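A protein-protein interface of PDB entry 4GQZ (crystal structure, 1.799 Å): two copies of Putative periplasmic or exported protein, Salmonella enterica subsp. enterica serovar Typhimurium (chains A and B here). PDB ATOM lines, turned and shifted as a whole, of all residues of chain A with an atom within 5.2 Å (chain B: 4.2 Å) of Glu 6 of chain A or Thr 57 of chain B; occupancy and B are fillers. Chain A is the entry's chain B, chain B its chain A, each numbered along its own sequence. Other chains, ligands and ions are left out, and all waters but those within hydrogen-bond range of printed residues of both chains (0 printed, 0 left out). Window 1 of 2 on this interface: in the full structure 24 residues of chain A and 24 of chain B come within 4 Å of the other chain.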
ATOM      1  N   SER A   4      17.886 -14.641  -6.525  1.00  0.00           N
ATOM      2  CA  SER A   4      18.173 -16.052  -6.772  1.00  0.00           C
ATOM      3  C   SER A   4      17.166 -16.981  -6.087  1.00  0.00           C
ATOM      4  O   SER A   4      16.440 -16.565  -5.176  1.00  0.00           O
ATOM      5  CB  SER A   4      19.572 -16.391  -6.282  1.00  0.00           C
ATOM      6  OG  SER A   4      19.691 -16.153  -4.887  1.00  0.00           O
ATOM      7  N   SER A   5      17.124 -18.241  -6.524  1.00  0.00           N
ATOM      8  CA  SER A   5      16.340 -19.259  -5.833  1.00  0.00           C
ATOM      9  C   SER A   5      16.803 -19.385  -4.391  1.00  0.00           C
ATOM     10  O   SER A   5      15.995 -19.610  -3.482  1.00  0.00           O
ATOM     11  CB  SER A   5      16.472 -20.618  -6.537  1.00  0.00           C
ATOM     12  OG  SER A   5      15.876 -20.589  -7.818  1.00  0.00           O
ATOM     13  N   GLU A   6      18.111 -19.245  -4.190  1.00  0.00           N
ATOM     14  CA  GLU A   6      18.703 -19.315  -2.860  1.00  0.00           C
ATOM     15  C   GLU A   6      18.160 -18.214  -1.976  1.00  0.00           C
ATOM     16  O   GLU A   6      17.732 -18.463  -0.839  1.00  0.00           O
ATOM     17  CB  GLU A   6      20.240 -19.238  -2.946  1.00  0.00           C
ATOM     18  CG  GLU A   6      20.953 -19.198  -1.578  1.00  0.00           C
ATOM     19  CD  GLU A   6      21.287 -17.778  -1.127  1.00  0.00           C
ATOM     20  OE1 GLU A   6      21.488 -16.911  -2.004  1.00  0.00           O
ATOM     21  OE2 GLU A   6      21.359 -17.533   0.107  1.00  0.00           O
ATOM     22  N   SER A   7      18.168 -16.990  -2.491  1.00  0.00           N
ATOM     23  CA  SER A   7      17.643 -15.862  -1.715  1.00  0.00           C
ATOM     24  C   SER A   7      16.164 -16.053  -1.411  1.00  0.00           C
ATOM     25  O   SER A   7      15.707 -15.798  -0.298  1.00  0.00           O
ATOM     26  CB  SER A   7      17.854 -14.549  -2.462  1.00  0.00           C
ATOM     27  OG  SER A   7      19.228 -14.220  -2.486  1.00  0.00           O
ATOM     28  N   ALA A   8      15.419 -16.531  -2.398  1.00  0.00           N
ATOM     29  CA  ALA A   8      13.994 -16.762  -2.191  1.00  0.00           C
ATOM     30  C   ALA A   8      13.728 -17.874  -1.163  1.00  0.00           C
ATOM     31  O   ALA A   8      12.791 -17.765  -0.368  1.00  0.00           O
ATOM     32  CB  ALA A   8      13.293 -17.049  -3.513  1.00  0.00           C
ATOM     33  N   PHE A   9      14.548 -18.929  -1.177  1.00  0.00           N
ATOM     34  CA  PHE A   9      14.430 -20.022  -0.204  1.00  0.00           C
ATOM     35  C   PHE A   9      14.538 -19.454   1.200  1.00  0.00           C
ATOM     36  O   PHE A   9      13.717 -19.749   2.061  1.00  0.00           O
ATOM     37  CB  PHE A   9      15.538 -21.065  -0.428  1.00  0.00           C
ATOM     38  CG  PHE A   9      15.502 -22.230   0.539  1.00  0.00           C
ATOM     39  CD1 PHE A   9      16.152 -22.156   1.756  1.00  0.00           C
ATOM     40  CD2 PHE A   9      14.828 -23.406   0.211  1.00  0.00           C
ATOM     41  CE1 PHE A   9      16.129 -23.218   2.647  1.00  0.00           C
ATOM     42  CE2 PHE A   9      14.802 -24.478   1.093  1.00  0.00           C
ATOM     43  CZ  PHE A   9      15.452 -24.380   2.315  1.00  0.00           C
ATOM     44  N   LEU A  10      15.561 -18.634   1.421  1.00  0.00           N
ATOM     45  CA  LEU A  10      15.757 -17.986   2.720  1.00  0.00           C
ATOM     46  C   LEU A  10      14.499 -17.236   3.178  1.00  0.00           C
ATOM     47  O   LEU A  10      14.036 -17.403   4.306  1.00  0.00           O
ATOM     48  CB  LEU A  10      16.971 -17.048   2.671  1.00  0.00           C
ATOM     49  CG  LEU A  10      18.314 -17.614   3.125  1.00  0.00           C
ATOM     50  CD1 LEU A  10      18.600 -18.916   2.461  1.00  0.00           C
ATOM     51  CD2 LEU A  10      19.434 -16.658   2.845  1.00  0.00           C
ATOM     52  N   TYR A  56      21.636 -25.292  -1.683  1.00  0.00           N
ATOM     53  CA  TYR A  56      22.196 -23.969  -1.447  1.00  0.00           C
ATOM     54  C   TYR A  56      23.216 -24.112  -0.350  1.00  0.00           C
ATOM     55  O   TYR A  56      23.032 -24.940   0.543  1.00  0.00           O
ATOM     56  CB  TYR A  56      21.099 -22.995  -1.014  1.00  0.00           C
ATOM     57  CG  TYR A  56      19.889 -23.029  -1.932  1.00  0.00           C
ATOM     58  CD1 TYR A  56      20.010 -22.723  -3.277  1.00  0.00           C
ATOM     59  CD2 TYR A  56      18.630 -23.375  -1.444  1.00  0.00           C
ATOM     60  CE1 TYR A  56      18.898 -22.768  -4.134  1.00  0.00           C
ATOM     61  CE2 TYR A  56      17.518 -23.420  -2.280  1.00  0.00           C
ATOM     62  CZ  TYR A  56      17.667 -23.114  -3.623  1.00  0.00           C
ATOM     63  OH  TYR A  56      16.567 -23.168  -4.439  1.00  0.00           O
ATOM     64  N   LEU A  58      25.509 -21.946   2.534  1.00  0.00           N
ATOM     65  CA  LEU A  58      25.777 -20.707   3.241  1.00  0.00           C
ATOM     66  C   LEU A  58      27.032 -20.906   4.077  1.00  0.00           C
ATOM     67  O   LEU A  58      27.083 -21.802   4.920  1.00  0.00           O
ATOM     68  CB  LEU A  58      24.607 -20.343   4.148  1.00  0.00           C
ATOM     69  CG  LEU A  58      23.206 -20.257   3.544  1.00  0.00           C
ATOM     70  CD1 LEU A  58      22.188 -19.819   4.597  1.00  0.00           C
ATOM     71  CD2 LEU A  58      23.169 -19.332   2.336  1.00  0.00           C
ATOM     72  N   GLU B   6      23.671 -20.459  -7.035  1.00  0.00           N
ATOM     73  CA  GLU B   6      24.439 -19.870  -5.934  1.00  0.00           C
ATOM     74  C   GLU B   6      25.663 -20.702  -5.535  1.00  0.00           C
ATOM     75  O   GLU B   6      26.758 -20.162  -5.386  1.00  0.00           O
ATOM     76  CB  GLU B   6      23.538 -19.641  -4.712  1.00  0.00           C
ATOM     77  CG  GLU B   6      24.255 -19.007  -3.524  1.00  0.00           C
ATOM     78  CD  GLU B   6      24.606 -19.995  -2.423  1.00  0.00           C
ATOM     79  OE1 GLU B   6      24.056 -21.120  -2.395  1.00  0.00           O
ATOM     80  OE2 GLU B   6      25.427 -19.623  -1.565  1.00  0.00           O
ATOM     81  N   GLU B  46      24.243  -9.060   5.862  1.00  0.00           N
ATOM     82  CA  GLU B  46      24.665 -10.006   4.825  1.00  0.00           C
ATOM     83  C   GLU B  46      25.576  -9.488   3.739  1.00  0.00           C
ATOM     84  O   GLU B  46      25.744  -8.284   3.560  1.00  0.00           O
ATOM     85  CB  GLU B  46      23.462 -10.671   4.174  1.00  0.00           C
ATOM     86  CG  GLU B  46      22.555  -9.690   3.559  1.00  0.00           C
ATOM     87  CD  GLU B  46      21.137  -9.896   4.017  1.00  0.00           C
ATOM     88  OE1 GLU B  46      20.837  -9.493   5.165  1.00  0.00           O
ATOM     89  OE2 GLU B  46      20.331 -10.462   3.233  1.00  0.00           O
ATOM     90  N   LEU B  47      26.152 -10.436   3.008  1.00  0.00           N
ATOM     91  CA  LEU B  47      26.924 -10.129   1.821  1.00  0.00           C
ATOM     92  C   LEU B  47      26.062 -10.444   0.606  1.00  0.00           C
ATOM     93  O   LEU B  47      25.523 -11.545   0.483  1.00  0.00           O
ATOM     94  CB  LEU B  47      28.210 -10.960   1.794  1.00  0.00           C
ATOM     95  CG  LEU B  47      29.040 -10.856   0.511  1.00  0.00           C
ATOM     96  CD1 LEU B  47      29.599  -9.458   0.365  1.00  0.00           C
ATOM     97  CD2 LEU B  47      30.174 -11.881   0.532  1.00  0.00           C
ATOM     98  N   TYR B  56      22.794 -13.275  -5.049  1.00  0.00           N
ATOM     99  CA  TYR B  56      22.918 -14.299  -4.019  1.00  0.00           C
ATOM    100  C   TYR B  56      23.156 -13.565  -2.716  1.00  0.00           C
ATOM    101  O   TYR B  56      23.779 -12.505  -2.709  1.00  0.00           O
ATOM    102  CB  TYR B  56      24.107 -15.201  -4.345  1.00  0.00           C
ATOM    103  CG  TYR B  56      24.067 -15.677  -5.783  1.00  0.00           C
ATOM    104  CD1 TYR B  56      23.104 -16.586  -6.194  1.00  0.00           C
ATOM    105  CD2 TYR B  56      24.958 -15.187  -6.731  1.00  0.00           C
ATOM    106  CE1 TYR B  56      23.041 -17.024  -7.503  1.00  0.00           C
ATOM    107  CE2 TYR B  56      24.898 -15.617  -8.054  1.00  0.00           C
ATOM    108  CZ  TYR B  56      23.934 -16.539  -8.429  1.00  0.00           C
ATOM    109  OH  TYR B  56      23.847 -16.986  -9.740  1.00  0.00           O
ATOM    110  N   THR B  57      22.649 -14.112  -1.617  1.00  0.00           N
ATOM    111  CA  THR B  57      22.781 -13.460  -0.324  1.00  0.00           C
ATOM    112  C   THR B  57      23.392 -14.416   0.678  1.00  0.00           C
ATOM    113  O   THR B  57      22.846 -15.498   0.938  1.00  0.00           O
ATOM    114  CB  THR B  57      21.415 -13.007   0.202  1.00  0.00           C
ATOM    115  OG1 THR B  57      20.495 -14.100   0.113  1.00  0.00           O
ATOM    116  CG2 THR B  57      20.877 -11.863  -0.644  1.00  0.00           C
ATOM    117  N   LEU B  58      24.528 -14.023   1.245  1.00  0.00           N
ATOM    118  CA  LEU B  58      25.191 -14.847   2.241  1.00  0.00           C
ATOM    119  C   LEU B  58      25.106 -14.124   3.582  1.00  0.00           C
ATOM    120  O   LEU B  58      25.692 -13.060   3.751  1.00  0.00           O
ATOM    121  CB  LEU B  58      26.661 -15.081   1.871  1.00  0.00           C
ATOM    122  CG  LEU B  58      27.061 -15.474   0.440  1.00  0.00           C
ATOM    123  CD1 LEU B  58      28.574 -15.697   0.318  1.00  0.00           C
ATOM    124  CD2 LEU B  58      26.325 -16.688  -0.064  1.00  0.00           C
ATOM    125  N   PRO B  59      24.364 -14.696   4.534  1.00  0.00           N
ATOM    126  CA  PRO B  59      24.254 -14.159   5.888  1.00  0.00           C
ATOM    127  C   PRO B  59      25.623 -13.962   6.521  1.00  0.00           C
ATOM    128  O   PRO B  59      26.491 -14.835   6.434  1.00  0.00           O
ATOM    129  CB  PRO B  59      23.499 -15.265   6.629  1.00  0.00           C
ATOM    130  CG  PRO B  59      22.637 -15.873   5.559  1.00  0.00           C
ATOM    131  CD  PRO B  59      23.526 -15.898   4.352  1.00  0.00           C
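The side-chain hydroxyl (OG1) of Thr 57 of chain B lies within hydrogen-bond range of the side-chain hydroxyl (OG) of Ser 7 of chain A, 2.9 Å away. OE1 of Glu 6 of chain A sits at hydrogen-bond distance from N of Thr 57 of chain B (3.1 Å).
Of chain B, only Glu 6, Tyr 56 and Thr 57 come within 4 Å of Glu 6 of chain A. Printed residues of chain B within 4 Å of Leu 10 of chain A: Thr 57 (3.9 Å). Printed residues of chain B within 4 Å of Tyr 56 of chain A: Glu 6. Of the printed residues of chain A, Glu 6 of chain B touches Glu 6 (3.7 Å) and Tyr 56 (3.5 Å). Thr 57 of chain B touches just these residues of chain A: Glu 6, Ser 7 and Leu 10.
Hydrophobic or aromatic side chains of chain A within 4 Å of the printed part of chain B: Leu 10, Tyr 56 and Leu 58. Of the 7 printed residues of chain B, 4 touch a printed residue of chain A. Hydrophobic or aromatic side chains of chain B that line the printed part of chain A: Tyr 56 and Pro 59. Among the printed residues, 9 pairs touch across the chains.
OG of Ser 4 of chain A is in hydrogen-bond range of N of Ser 7 of chain A, 3.0 Å away. The side-chain carboxylate (OE1) of Glu 6 of chain A sits at hydrogen-bond distance from the side-chain hydroxyl (OG) of Ser 4 of chain A (3.5 Å).
Among the printed residues, merely in contact across the chains: Ser 4 of chain A with Tyr 56 of chain B (3.5 Å), Glu 6 of chain A with Glu 6 of chain B (3.7 Å), Glu 6 of chain A with Tyr 56 of chain B (3.6 Å), Ser 7 of chain A with Tyr 56 of chain B (3.99 Å), Leu 10 of chain A with Thr 57 of chain B (3.9 Å), Tyr 56 of chain A with Glu 6 of chain B (3.5 Å) and Leu 58 of chain A with Pro 59 of chain B (3.998 Å).
Glu 6 of chain A touches its own counterpart, Glu 6 of chain B. Glu 6 of chain A touches Tyr 56 of chain B, and with the chains exchanged Tyr 56 of chain A touches Glu 6 of chain B.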
